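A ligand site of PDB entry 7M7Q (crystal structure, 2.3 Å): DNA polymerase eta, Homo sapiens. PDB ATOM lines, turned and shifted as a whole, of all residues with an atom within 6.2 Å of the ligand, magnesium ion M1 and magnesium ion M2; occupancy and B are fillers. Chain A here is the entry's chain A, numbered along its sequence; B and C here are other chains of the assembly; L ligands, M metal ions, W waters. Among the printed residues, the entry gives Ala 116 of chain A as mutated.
An oxygen (O5) of the ligand is in hydrogen-bond range of the backbone NH (N) of Phe 20, 3.3 Å away.
N3 of the ligand sits at hydrogen-bond distance from O4 of DT 4 of chain C, at 3.0 Å.
NH1 of Arg 64 is in salt-bridge range of O4 of the ligand, at 3.2 Å.
An oxygen (O6) of the ligand sits at hydrogen-bond distance from the backbone NH of Cys 19, 2.8 Å away.
NZ of Lys 234 lies within salt-bridge range of O6 of the ligand.
O6 of the ligand sits at hydrogen-bond distance from OH of Tyr 55, 2.7 Å away.
N of Phe 21 sits at hydrogen-bond distance from O7 of the ligand.
NH1 of Arg 58 is in salt-bridge range of O9 of the ligand (3.0 Å).
N3 of DT 9 of chain B sits at hydrogen-bond distance from N3 of the ligand.
OH of Tyr 55 lies within hydrogen-bond range of NH1 of Arg 58 (3.3 Å).
NE of Arg 58 lies within hydrogen-bond range of O of Val 53, 2.9 Å away.
The backbone carbonyl oxygen (O) of Asp 16 is in hydrogen-bond range of the side-chain amino group (NZ) of Lys 234 (3.0 Å).
NZ of Lys 227 lies close to OD2 of Asp 16 (3.9 Å).
The side-chain amide nitrogen of Gln 41 lies within hydrogen-bond range of O4' of DT 4 of chain C (3.1 Å).
The side-chain amino group of Lys 234 is in salt-bridge range of the side-chain carboxylate of Asp 18 (2.8 Å).
N3 of DT 9 of chain B lies close to N1 of DA 5 of chain C (2.7 Å).
O of Met 17 sits close to NZ of Lys 234 (3.0 Å).
CA of Asp 18 touches O6 of the ligand, at 3.2 Å.
Ile 51 touches the ligand (O to C7, 3.3 Å).
Ala 52 touches the ligand.
Ile 117 touches the ligand.
DA 5 of chain C touches the ligand (N1 to N1, 3.6 Å).
Hydrophobic or aromatic side chains within 4 Å of the ligand: Phe 20, Phe 21, Ala 52, Tyr 55 and Ile 117.
Of the 25 residues printed, 17 come within 4 Å of the ligand.
NZ of Lys 234 touches magnesium ion M1, at 3.7 Å.
Four residues have an atom within 4 Å of magnesium ion M1: Asp 16, Met 17, Asp 118 and Lys 234.
The nearest printed residue that does not touch magnesium ion M1 is Asp 18 (4.4 Å).
Of the 25 residues printed, 4 come within 4 Å of magnesium ion M2.
Magnesium ion M1 is bound by O3 of the ligand.
Magnesium ion M1 is bound by O2 of the ligand, at 2.1 Å.
The side-chain carboxylate (OD1) of Asp 16 binds magnesium ion M1, at 2.2 Å.
The backbone carbonyl oxygen (O) of Met 17 is bound to magnesium ion M1 (2.2 Å).
The side-chain carboxylate (OD2) of Asp 118 is bound to magnesium ion M1 (2.3 Å).
O1 of the ligand is bound to magnesium ion M1 (2.3 Å).
Magnesium ion M1 has six donor atoms within binding distance.
Magnesium ion M2 is bound by the side-chain carboxylate (OD2) of Asp 16 (2.1 Å), water W9 (2.1 Å), an oxygen (O1) of the ligand (2.2 Å), the side-chain carboxylate (OD1) of Asp 118 (2.2 Å), the side-chain carboxylate (OE2) of Glu 119 (2.2 Å) and O3' of DT 9 of chain B (2.3 Å).
Magnesium ion M2 has six donor atoms within binding distance.
Water W9 lies within hydrogen-bond range of an oxygen (O4) of the ligand (3.2 Å) and the side-chain amino group (NZ) of Lys 227 (3.2 Å).
Water W5 lies within hydrogen-bond range of an oxygen (O5) of the ligand, the backbone NH (N) of Val 53 and the guanidinium group (NH2) of Arg 58.
Water W1 bridges N3 of the ligand (3.0 Å) and NE of Arg 64 (3.3 Å).
Water W2 lies within hydrogen-bond range of NH1 of Arg 64 (2.6 Å), N6 of the ligand (3.0 Å) and O of Ile 51 (3.1 Å).
Water W6 lies within hydrogen-bond range of O2 of DT 9 of chain B (2.7 Å) and O10 of the ligand (3.3 Å).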
ATOM      1  N   ASP A  16      -8.701   1.282  25.808  1.00  0.00           N
ATOM      2  CA  ASP A  16      -9.409   0.923  24.595  1.00  0.00           C
ATOM      3  C   ASP A  16      -8.426   0.521  23.490  1.00  0.00           C
ATOM      4  O   ASP A  16      -7.523   1.288  23.146  1.00  0.00           O
ATOM      5  CB  ASP A  16     -10.270   2.097  24.120  1.00  0.00           C
ATOM      6  CG  ASP A  16     -11.124   1.731  22.960  1.00  0.00           C
ATOM      7  OD1 ASP A  16     -10.603   1.740  21.845  1.00  0.00           O
ATOM      8  OD2 ASP A  16     -12.309   1.426  23.153  1.00  0.00           O
ATOM      9  N   MET A  17      -8.638  -0.644  22.911  1.00  0.00           N
ATOM     10  CA  MET A  17      -7.718  -1.174  21.927  1.00  0.00           C
ATOM     11  C   MET A  17      -7.753  -0.343  20.637  1.00  0.00           C
ATOM     12  O   MET A  17      -8.809   0.143  20.210  1.00  0.00           O
ATOM     13  CB  MET A  17      -8.087  -2.628  21.627  1.00  0.00           C
ATOM     14  CG  MET A  17      -8.172  -3.537  22.856  1.00  0.00           C
ATOM     15  SD  MET A  17      -6.762  -3.434  23.998  1.00  0.00           S
ATOM     16  CE  MET A  17      -5.517  -4.251  23.013  1.00  0.00           C
ATOM     17  N   ASP A  18      -6.586  -0.165  20.030  1.00  0.00           N
ATOM     18  CA  ASP A  18      -6.543   0.544  18.758  1.00  0.00           C
ATOM     19  C   ASP A  18      -7.004  -0.412  17.664  1.00  0.00           C
ATOM     20  O   ASP A  18      -6.543  -1.556  17.622  1.00  0.00           O
ATOM     21  CB  ASP A  18      -5.117   1.025  18.512  1.00  0.00           C
ATOM     22  CG  ASP A  18      -4.642   2.011  19.593  1.00  0.00           C
ATOM     23  OD1 ASP A  18      -5.498   2.739  20.166  1.00  0.00           O
ATOM     24  OD2 ASP A  18      -3.419   2.057  19.862  1.00  0.00           O
ATOM     25  N   CYS A  19      -7.891   0.072  16.777  1.00  0.00           N
ATOM     26  CA  CYS A  19      -8.477  -0.696  15.660  1.00  0.00           C
ATOM     27  C   CYS A  19      -8.496  -2.209  15.962  1.00  0.00           C
ATOM     28  O   CYS A  19      -7.871  -2.993  15.255  1.00  0.00           O
ATOM     29  CB  CYS A  19      -7.740  -0.406  14.343  1.00  0.00           C
ATOM     30  SG  CYS A  19      -5.916  -0.581  14.329  1.00  0.00           S
ATOM     31  N   PHE A  20      -9.261  -2.594  16.989  1.00  0.00           N
ATOM     32  CA  PHE A  20      -9.110  -3.914  17.634  1.00  0.00           C
ATOM     33  C   PHE A  20      -9.216  -5.104  16.670  1.00  0.00           C
ATOM     34  O   PHE A  20      -8.296  -5.928  16.586  1.00  0.00           O
ATOM     35  CB  PHE A  20     -10.109  -4.047  18.773  1.00  0.00           C
ATOM     36  CG  PHE A  20      -9.932  -5.292  19.566  1.00  0.00           C
ATOM     37  CD1 PHE A  20      -8.672  -5.658  20.007  1.00  0.00           C
ATOM     38  CD2 PHE A  20     -11.014  -6.090  19.878  1.00  0.00           C
ATOM     39  CE1 PHE A  20      -8.476  -6.820  20.739  1.00  0.00           C
ATOM     40  CE2 PHE A  20     -10.828  -7.252  20.620  1.00  0.00           C
ATOM     41  CZ  PHE A  20      -9.559  -7.617  21.051  1.00  0.00           C
ATOM     42  N   PHE A  21     -10.318  -5.230  15.913  1.00  0.00           N
ATOM     43  CA  PHE A  21     -10.469  -6.432  15.086  1.00  0.00           C
ATOM     44  C   PHE A  21      -9.357  -6.489  14.043  1.00  0.00           C
ATOM     45  O   PHE A  21      -8.859  -7.573  13.686  1.00  0.00           O
ATOM     46  CB  PHE A  21     -11.829  -6.481  14.369  1.00  0.00           C
ATOM     47  CG  PHE A  21     -13.013  -6.758  15.277  1.00  0.00           C
ATOM     48  CD1 PHE A  21     -12.902  -6.692  16.650  1.00  0.00           C
ATOM     49  CD2 PHE A  21     -14.260  -7.049  14.718  1.00  0.00           C
ATOM     50  CE1 PHE A  21     -14.026  -6.928  17.483  1.00  0.00           C
ATOM     51  CE2 PHE A  21     -15.379  -7.285  15.526  1.00  0.00           C
ATOM     52  CZ  PHE A  21     -15.264  -7.225  16.920  1.00  0.00           C
ATOM     53  N   VAL A  22      -8.928  -5.317  13.558  1.00  0.00           N
ATOM     54  CA  VAL A  22      -7.819  -5.271  12.605  1.00  0.00           C
ATOM     55  C   VAL A  22      -6.536  -5.806  13.236  1.00  0.00           C
ATOM     56  O   VAL A  22      -5.855  -6.663  12.645  1.00  0.00           O
ATOM     57  CB  VAL A  22      -7.635  -3.845  12.056  1.00  0.00           C
ATOM     58  CG1 VAL A  22      -6.296  -3.716  11.357  1.00  0.00           C
ATOM     59  CG2 VAL A  22      -8.762  -3.517  11.085  1.00  0.00           C
ATOM     60  N   GLN A  41     -17.574  -7.878   7.091  1.00  0.00           N
ATOM     61  CA  GLN A  41     -18.442  -9.027   7.276  1.00  0.00           C
ATOM     62  C   GLN A  41     -19.322  -9.162   6.047  1.00  0.00           C
ATOM     63  O   GLN A  41     -19.834  -8.157   5.537  1.00  0.00           O
ATOM     64  CB  GLN A  41     -19.300  -8.932   8.542  1.00  0.00           C
ATOM     65  CG  GLN A  41     -19.951  -7.626   8.772  1.00  0.00           C
ATOM     66  CD  GLN A  41     -20.573  -7.589  10.148  1.00  0.00           C
ATOM     67  OE1 GLN A  41     -20.211  -8.381  11.041  1.00  0.00           O
ATOM     68  NE2 GLN A  41     -21.523  -6.688  10.325  1.00  0.00           N
ATOM     69  N   ILE A  51     -16.236  -3.111   9.448  1.00  0.00           N
ATOM     70  CA  ILE A  51     -16.477  -2.888  10.872  1.00  0.00           C
ATOM     71  C   ILE A  51     -15.242  -2.433  11.629  1.00  0.00           C
ATOM     72  O   ILE A  51     -15.372  -2.076  12.816  1.00  0.00           O
ATOM     73  CB  ILE A  51     -17.096  -4.119  11.555  1.00  0.00           C
ATOM     74  CG1 ILE A  51     -16.176  -5.336  11.437  1.00  0.00           C
ATOM     75  CG2 ILE A  51     -18.496  -4.376  10.990  1.00  0.00           C
ATOM     76  CD1 ILE A  51     -16.681  -6.531  12.236  1.00  0.00           C
ATOM     77  N   ALA A  52     -14.054  -2.492  11.048  1.00  0.00           N
ATOM     78  CA  ALA A  52     -12.865  -1.981  11.716  1.00  0.00           C
ATOM     79  C   ALA A  52     -11.856  -1.582  10.653  1.00  0.00           C
ATOM     80  O   ALA A  52     -11.795  -2.225   9.607  1.00  0.00           O
ATOM     81  CB  ALA A  52     -12.280  -3.029  12.681  1.00  0.00           C
ATOM     82  N   VAL A  53     -11.057  -0.556  10.945  1.00  0.00           N
ATOM     83  CA  VAL A  53     -10.215   0.095   9.940  1.00  0.00           C
ATOM     84  C   VAL A  53      -8.859   0.452  10.549  1.00  0.00           C
ATOM     85  O   VAL A  53      -8.800   1.110  11.596  1.00  0.00           O
ATOM     86  CB  VAL A  53     -10.873   1.391   9.404  1.00  0.00           C
ATOM     87  CG1 VAL A  53     -10.063   1.955   8.254  1.00  0.00           C
ATOM     88  CG2 VAL A  53     -12.278   1.143   8.947  1.00  0.00           C
ATOM     89  N   TYR A  55      -5.279   2.435  10.994  1.00  0.00           N
ATOM     90  CA  TYR A  55      -5.033   3.875  10.903  1.00  0.00           C
ATOM     91  C   TYR A  55      -4.455   4.263   9.553  1.00  0.00           C
ATOM     92  O   TYR A  55      -4.795   5.318   8.987  1.00  0.00           O
ATOM     93  CB  TYR A  55      -4.143   4.342  12.057  1.00  0.00           C
ATOM     94  CG  TYR A  55      -4.962   4.482  13.323  1.00  0.00           C
ATOM     95  CD1 TYR A  55      -5.319   3.351  14.076  1.00  0.00           C
ATOM     96  CD2 TYR A  55      -5.488   5.708  13.697  1.00  0.00           C
ATOM     97  CE1 TYR A  55      -6.130   3.454  15.189  1.00  0.00           C
ATOM     98  CE2 TYR A  55      -6.287   5.822  14.821  1.00  0.00           C
ATOM     99  CZ  TYR A  55      -6.622   4.694  15.565  1.00  0.00           C
ATOM    100  OH  TYR A  55      -7.435   4.801  16.694  1.00  0.00           O
ATOM    101  N   ARG A  58      -7.420   4.581   7.459  1.00  0.00           N
ATOM    102  CA  ARG A  58      -8.200   5.771   7.812  1.00  0.00           C
ATOM    103  C   ARG A  58      -7.632   7.020   7.163  1.00  0.00           C
ATOM    104  O   ARG A  58      -8.370   7.980   6.893  1.00  0.00           O
ATOM    105  CB  ARG A  58      -8.261   5.971   9.329  1.00  0.00           C
ATOM    106  CG  ARG A  58      -8.963   4.871  10.101  1.00  0.00           C
ATOM    107  CD  ARG A  58      -8.932   5.102  11.614  1.00  0.00           C
ATOM    108  NE  ARG A  58      -9.256   3.842  12.310  1.00  0.00           N
ATOM    109  CZ  ARG A  58      -9.611   3.734  13.584  1.00  0.00           C
ATOM    110  NH1 ARG A  58      -9.699   4.803  14.357  1.00  0.00           N
ATOM    111  NH2 ARG A  58      -9.868   2.535  14.082  1.00  0.00           N
ATOM    112  N   ARG A  64     -15.613   2.947   9.356  1.00  0.00           N
ATOM    113  CA  ARG A  64     -16.616   1.957   9.747  1.00  0.00           C
ATOM    114  C   ARG A  64     -17.949   2.224   9.032  1.00  0.00           C
ATOM    115  O   ARG A  64     -18.310   3.375   8.789  1.00  0.00           O
ATOM    116  CB  ARG A  64     -16.813   2.037  11.270  1.00  0.00           C
ATOM    117  CG  ARG A  64     -17.711   0.977  11.871  1.00  0.00           C
ATOM    118  CD  ARG A  64     -17.671   1.087  13.383  1.00  0.00           C
ATOM    119  NE  ARG A  64     -17.701   2.484  13.807  1.00  0.00           N
ATOM    120  CZ  ARG A  64     -17.046   2.964  14.865  1.00  0.00           C
ATOM    121  NH1 ARG A  64     -16.315   2.162  15.632  1.00  0.00           N
ATOM    122  NH2 ARG A  64     -17.134   4.261  15.169  1.00  0.00           N
ATOM    123  N   ALA A 116     -16.937  -2.761  26.748  1.00  0.00           N
ATOM    124  CA  ALA A 116     -17.262  -3.273  25.427  1.00  0.00           C
ATOM    125  C   ALA A 116     -16.203  -4.330  25.069  1.00  0.00           C
ATOM    126  O   ALA A 116     -15.211  -4.502  25.801  1.00  0.00           O
ATOM    127  CB  ALA A 116     -17.323  -2.142  24.398  1.00  0.00           C
ATOM    128  N   ILE A 117     -16.381  -4.979  23.915  1.00  0.00           N
ATOM    129  CA  ILE A 117     -15.493  -6.066  23.514  1.00  0.00           C
ATOM    130  C   ILE A 117     -14.031  -5.616  23.564  1.00  0.00           C
ATOM    131  O   ILE A 117     -13.132  -6.418  23.834  1.00  0.00           O
ATOM    132  CB  ILE A 117     -15.853  -6.614  22.123  1.00  0.00           C
ATOM    133  CG1 ILE A 117     -15.196  -7.990  21.930  1.00  0.00           C
ATOM    134  CG2 ILE A 117     -15.337  -5.704  21.060  1.00  0.00           C
ATOM    135  CD1 ILE A 117     -15.835  -8.826  20.817  1.00  0.00           C
ATOM    136  N   ASP A 118     -13.752  -4.311  23.426  1.00  0.00           N
ATOM    137  CA  ASP A 118     -12.350  -3.904  23.386  1.00  0.00           C
ATOM    138  C   ASP A 118     -12.017  -2.789  24.358  1.00  0.00           C
ATOM    139  O   ASP A 118     -11.000  -2.115  24.184  1.00  0.00           O
ATOM    140  CB  ASP A 118     -11.914  -3.417  21.980  1.00  0.00           C
ATOM    141  CG  ASP A 118     -12.256  -1.910  21.719  1.00  0.00           C
ATOM    142  OD1 ASP A 118     -13.188  -1.334  22.345  1.00  0.00           O
ATOM    143  OD2 ASP A 118     -11.404  -1.224  21.093  1.00  0.00           O
ATOM    144  N   GLU A 119     -12.853  -2.571  25.367  1.00  0.00           N
ATOM    145  CA  GLU A 119     -12.498  -1.535  26.332  1.00  0.00           C
ATOM    146  C   GLU A 119     -12.999  -1.876  27.714  1.00  0.00           C
ATOM    147  O   GLU A 119     -14.064  -2.513  27.860  1.00  0.00           O
ATOM    148  CB  GLU A 119     -12.983  -0.147  25.913  1.00  0.00           C
ATOM    149  CG  GLU A 119     -14.459   0.031  25.996  1.00  0.00           C
ATOM    150  CD  GLU A 119     -14.919   1.135  25.075  1.00  0.00           C
ATOM    151  OE1 GLU A 119     -15.083   2.259  25.604  1.00  0.00           O
ATOM    152  OE2 GLU A 119     -15.003   0.929  23.851  1.00  0.00           O
ATOM    153  N   LYS A 227     -12.873   8.162  29.580  1.00  0.00           N
ATOM    154  CA  LYS A 227     -13.288   7.806  28.215  1.00  0.00           C
ATOM    155  C   LYS A 227     -12.984   8.942  27.234  1.00  0.00           C
ATOM    156  O   LYS A 227     -12.410   8.710  26.170  1.00  0.00           O
ATOM    157  CB  LYS A 227     -14.790   7.456  28.223  1.00  0.00           C
ATOM    158  CG  LYS A 227     -15.449   7.155  26.870  1.00  0.00           C
ATOM    159  CD  LYS A 227     -14.586   6.195  26.034  1.00  0.00           C
ATOM    160  CE  LYS A 227     -15.319   5.503  24.855  1.00  0.00           C
ATOM    161  NZ  LYS A 227     -14.392   4.535  24.146  1.00  0.00           N
ATOM    162  N   LYS A 234      -5.275   8.882  20.634  1.00  0.00           N
ATOM    163  CA  LYS A 234      -5.183   7.634  19.877  1.00  0.00           C
ATOM    164  C   LYS A 234      -4.442   7.866  18.567  1.00  0.00           C
ATOM    165  O   LYS A 234      -4.636   8.905  17.918  1.00  0.00           O
ATOM    166  CB  LYS A 234      -6.588   7.100  19.581  1.00  0.00           C
ATOM    167  CG  LYS A 234      -7.198   6.269  20.654  1.00  0.00           C
ATOM    168  CD  LYS A 234      -8.455   5.547  20.171  1.00  0.00           C
ATOM    169  CE  LYS A 234      -8.856   4.426  21.165  1.00  0.00           C
ATOM    170  NZ  LYS A 234      -8.243   3.079  20.799  1.00  0.00           N
ATOM    171  N   PRO A 235      -3.641   6.883  18.083  1.00  0.00           N
ATOM    172  CA  PRO A 235      -3.470   5.593  18.766  1.00  0.00           C
ATOM    173  C   PRO A 235      -2.167   5.451  19.558  1.00  0.00           C
ATOM    174  O   PRO A 235      -1.280   6.298  19.474  1.00  0.00           O
ATOM    175  CB  PRO A 235      -3.418   4.593  17.599  1.00  0.00           C
ATOM    176  CG  PRO A 235      -2.653   5.396  16.522  1.00  0.00           C
ATOM    177  CD  PRO A 235      -3.091   6.852  16.703  1.00  0.00           C
ATOM    178  P    DT B   9     -19.104   4.613  21.937  1.00  0.00           P
ATOM    179  OP1  DT B   9     -17.947   5.385  22.434  1.00  0.00           O
ATOM    180  OP2  DT B   9     -19.780   5.005  20.666  1.00  0.00           O
ATOM    181  O5'  DT B   9     -18.685   3.086  21.727  1.00  0.00           O
ATOM    182  C5'  DT B   9     -18.362   2.229  22.831  1.00  0.00           C
ATOM    183  C4'  DT B   9     -17.919   0.889  22.286  1.00  0.00           C
ATOM    184  O4'  DT B   9     -19.079   0.181  21.737  1.00  0.00           O
ATOM    185  C3'  DT B   9     -16.911   1.000  21.143  1.00  0.00           C
ATOM    186  O3'  DT B   9     -15.930   0.015  21.272  1.00  0.00           O
ATOM    187  C2'  DT B   9     -17.744   0.806  19.876  1.00  0.00           C
ATOM    188  C1'  DT B   9     -18.848  -0.130  20.370  1.00  0.00           C
ATOM    189  N1   DT B   9     -20.129   0.008  19.615  1.00  0.00           N
ATOM    190  C2   DT B   9     -20.730  -1.125  19.101  1.00  0.00           C
ATOM    191  O2   DT B   9     -20.253  -2.231  19.242  1.00  0.00           O
ATOM    192  N3   DT B   9     -21.892  -0.921  18.423  1.00  0.00           N
ATOM    193  C4   DT B   9     -22.521   0.279  18.209  1.00  0.00           C
ATOM    194  O4   DT B   9     -23.575   0.351  17.583  1.00  0.00           O
ATOM    195  C5   DT B   9     -21.859   1.445  18.768  1.00  0.00           C
ATOM    196  C7   DT B   9     -22.456   2.814  18.586  1.00  0.00           C
ATOM    197  C6   DT B   9     -20.711   1.263  19.436  1.00  0.00           C
ATOM    198  P    DT C   3     -27.705   0.895   4.233  1.00  0.00           P
ATOM    199  OP1  DT C   3     -28.974   1.637   4.453  1.00  0.00           O
ATOM    200  OP2  DT C   3     -26.617   1.544   3.507  1.00  0.00           O
ATOM    201  O5'  DT C   3     -27.119   0.477   5.650  1.00  0.00           O
ATOM    202  C5'  DT C   3     -25.751   0.038   5.760  1.00  0.00           C
ATOM    203  C4'  DT C   3     -25.581  -0.981   6.861  1.00  0.00           C
ATOM    204  O4'  DT C   3     -24.671  -0.463   7.841  1.00  0.00           O
ATOM    205  C3'  DT C   3     -26.852  -1.315   7.627  1.00  0.00           C
ATOM    206  O3'  DT C   3     -26.795  -2.624   8.193  1.00  0.00           O
ATOM    207  C2'  DT C   3     -26.841  -0.314   8.763  1.00  0.00           C
ATOM    208  C1'  DT C   3     -25.362  -0.092   9.021  1.00  0.00           C
ATOM    209  N1   DT C   3     -25.026   1.307   9.327  1.00  0.00           N
ATOM    210  C2   DT C   3     -24.042   1.566  10.245  1.00  0.00           C
ATOM    211  O2   DT C   3     -23.403   0.680  10.798  1.00  0.00           O
ATOM    212  N3   DT C   3     -23.803   2.890  10.482  1.00  0.00           N
ATOM    213  C4   DT C   3     -24.457   3.966   9.895  1.00  0.00           C
ATOM    214  O4   DT C   3     -24.123   5.105  10.205  1.00  0.00           O
ATOM    215  C5   DT C   3     -25.488   3.623   8.957  1.00  0.00           C
ATOM    216  C7   DT C   3     -26.250   4.722   8.274  1.00  0.00           C
ATOM    217  C6   DT C   3     -25.723   2.329   8.718  1.00  0.00           C
ATOM    218  P    DT C   4     -27.567  -3.825   7.494  1.00  0.00           P
ATOM    219  OP1  DT C   4     -27.219  -3.813   6.058  1.00  0.00           O
ATOM    220  OP2  DT C   4     -28.983  -3.752   7.895  1.00  0.00           O
ATOM    221  O5'  DT C   4     -26.897  -5.099   8.160  1.00  0.00           O
ATOM    222  C5'  DT C   4     -25.536  -5.432   7.857  1.00  0.00           C
ATOM    223  C4'  DT C   4     -24.884  -6.137   9.028  1.00  0.00           C
ATOM    224  O4'  DT C   4     -24.174  -5.180   9.850  1.00  0.00           O
ATOM    225  C3'  DT C   4     -25.815  -6.892   9.969  1.00  0.00           C
ATOM    226  O3'  DT C   4     -25.183  -8.150  10.227  1.00  0.00           O
ATOM    227  C2'  DT C   4     -25.877  -5.998  11.193  1.00  0.00           C
ATOM    228  C1'  DT C   4     -24.481  -5.430  11.198  1.00  0.00           C
ATOM    229  N1   DT C   4     -24.297  -4.166  11.937  1.00  0.00           N
ATOM    230  C2   DT C   4     -23.148  -4.053  12.677  1.00  0.00           C
ATOM    231  O2   DT C   4     -22.312  -4.933  12.767  1.00  0.00           O
ATOM    232  N3   DT C   4     -23.008  -2.843  13.320  1.00  0.00           N
ATOM    233  C4   DT C   4     -23.875  -1.770  13.285  1.00  0.00           C
ATOM    234  O4   DT C   4     -23.619  -0.764  13.925  1.00  0.00           O
ATOM    235  C5   DT C   4     -25.065  -1.971  12.485  1.00  0.00           C
ATOM    236  C7   DT C   4     -26.078  -0.874  12.412  1.00  0.00           C
ATOM    237  C6   DT C   4     -25.210  -3.136  11.851  1.00  0.00           C
ATOM    238  P    DA C   5     -25.840  -9.296  11.171  1.00  0.00           P
ATOM    239  OP1  DA C   5     -25.535 -10.594  10.578  1.00  0.00           O
ATOM    240  OP2  DA C   5     -27.232  -8.965  11.493  1.00  0.00           O
ATOM    241  O5'  DA C   5     -25.014  -9.179  12.518  1.00  0.00           O
ATOM    242  C5'  DA C   5     -23.606  -9.462  12.536  1.00  0.00           C
ATOM    243  C4'  DA C   5     -23.101  -9.383  13.954  1.00  0.00           C
ATOM    244  O4'  DA C   5     -23.025  -8.000  14.354  1.00  0.00           O
ATOM    245  C3'  DA C   5     -23.960 -10.083  14.996  1.00  0.00           C
ATOM    246  O3'  DA C   5     -23.090 -10.760  15.899  1.00  0.00           O
ATOM    247  C2'  DA C   5     -24.693  -8.948  15.679  1.00  0.00           C
ATOM    248  C1'  DA C   5     -23.682  -7.818  15.584  1.00  0.00           C
ATOM    249  N9   DA C   5     -24.273  -6.487  15.589  1.00  0.00           N
ATOM    250  C8   DA C   5     -25.404  -6.043  14.956  1.00  0.00           C
ATOM    251  N7   DA C   5     -25.658  -4.775  15.155  1.00  0.00           N
ATOM    252  C5   DA C   5     -24.618  -4.348  15.968  1.00  0.00           C
ATOM    253  C6   DA C   5     -24.309  -3.100  16.534  1.00  0.00           C
ATOM    254  N6   DA C   5     -25.046  -2.003  16.369  1.00  0.00           N
ATOM    255  N1   DA C   5     -23.206  -3.021  17.306  1.00  0.00           N
ATOM    256  C2   DA C   5     -22.463  -4.118  17.485  1.00  0.00           C
ATOM    257  N3   DA C   5     -22.653  -5.347  17.011  1.00  0.00           N
ATOM    258  C4   DA C   5     -23.760  -5.398  16.248  1.00  0.00           C
HETATM  259  N1  LIG L   1     -20.751  -2.539  14.753  1.00  0.00           N
HETATM  260  C1  LIG L   1     -19.997  -3.640  14.830  1.00  0.00           C
HETATM  261  N2  LIG L   1     -18.807  -3.805  15.378  1.00  0.00           N
HETATM  262  C2  LIG L   1     -18.368  -2.661  15.905  1.00  0.00           C
HETATM  263  C3  LIG L   1     -19.008  -1.443  15.906  1.00  0.00           C
HETATM  264  C4  LIG L   1     -20.271  -1.399  15.296  1.00  0.00           C
HETATM  265  N3  LIG L   1     -20.980  -0.278  15.240  1.00  0.00           N
HETATM  266  N4  LIG L   1     -18.228  -0.489  16.545  1.00  0.00           N
HETATM  267  C5  LIG L   1     -17.154  -1.141  16.899  1.00  0.00           C
HETATM  268  N5  LIG L   1     -17.178  -2.463  16.539  1.00  0.00           N
HETATM  269  P1  LIG L   1     -13.919   0.741  18.599  1.00  0.00           P
HETATM  270  P2  LIG L   1     -11.552   0.278  16.984  1.00  0.00           P
HETATM  271  P3  LIG L   1     -10.128   2.725  17.658  1.00  0.00           P
HETATM  272  C6  LIG L   1     -16.167  -3.493  16.763  1.00  0.00           C
HETATM  273  O1  LIG L   1     -13.222   0.838  19.865  1.00  0.00           O
HETATM  274  O2  LIG L   1     -11.011  -0.435  18.135  1.00  0.00           O
HETATM  275  O3  LIG L   1     -10.688   2.414  18.994  1.00  0.00           O
HETATM  276  C7  LIG L   1     -15.031  -3.520  15.771  1.00  0.00           C
HETATM  277  O4  LIG L   1     -15.067   1.776  18.538  1.00  0.00           O
HETATM  278  O5  LIG L   1     -11.557  -0.656  15.748  1.00  0.00           O
HETATM  279  O6  LIG L   1      -8.663   2.632  17.639  1.00  0.00           O
HETATM  280  C8  LIG L   1     -13.933  -2.745  16.477  1.00  0.00           C
HETATM  281  O7  LIG L   1     -12.635  -3.216  16.138  1.00  0.00           O
HETATM  282  N6  LIG L   1     -12.998   0.912  17.277  1.00  0.00           N
HETATM  283  O8  LIG L   1     -10.678   1.568  16.705  1.00  0.00           O
HETATM  284  O9  LIG L   1     -10.631   4.004  17.104  1.00  0.00           O
HETATM  285  C9  LIG L   1     -14.202  -3.023  17.947  1.00  0.00           C
HETATM  286  O10 LIG L   1     -15.603  -3.332  18.061  1.00  0.00           O
HETATM  287  C10 LIG L   1     -13.862  -1.889  18.871  1.00  0.00           C
HETATM  288  O11 LIG L   1     -14.573  -0.698  18.477  1.00  0.00           O
HETATM  289 MG    MG M   1     -10.915   0.711  19.946  1.00  0.00          MG
HETATM  290 MG    MG M   2     -13.864   0.739  21.943  1.00  0.00          MG
HETATM  291  O   HOH W   1     -19.872   2.271  16.231  1.00  0.00           O
HETATM  292  O   HOH W   2     -14.706   0.211  14.866  1.00  0.00           O
HETATM  293  O   HOH W   3     -13.031   3.848  15.841  1.00  0.00           O
HETATM  294  O   HOH W   4     -15.530   4.412  18.361  1.00  0.00           O
HETATM  295  O   HOH W   5     -11.773   0.531  13.420  1.00  0.00           O
HETATM  296  O   HOH W   6     -18.659  -4.337  18.987  1.00  0.00           O
HETATM  297  O   HOH W   7     -12.295   4.109  20.183  1.00  0.00           O
HETATM  298  O   HOH W   8     -16.445  -2.593  20.661  1.00  0.00           O
HETATM  299  O   HOH W   9     -14.214   2.794  21.452  1.00  0.00           O
HETATM  300  O   HOH W  10     -18.612  -6.626  15.647  1.00  0.00           O
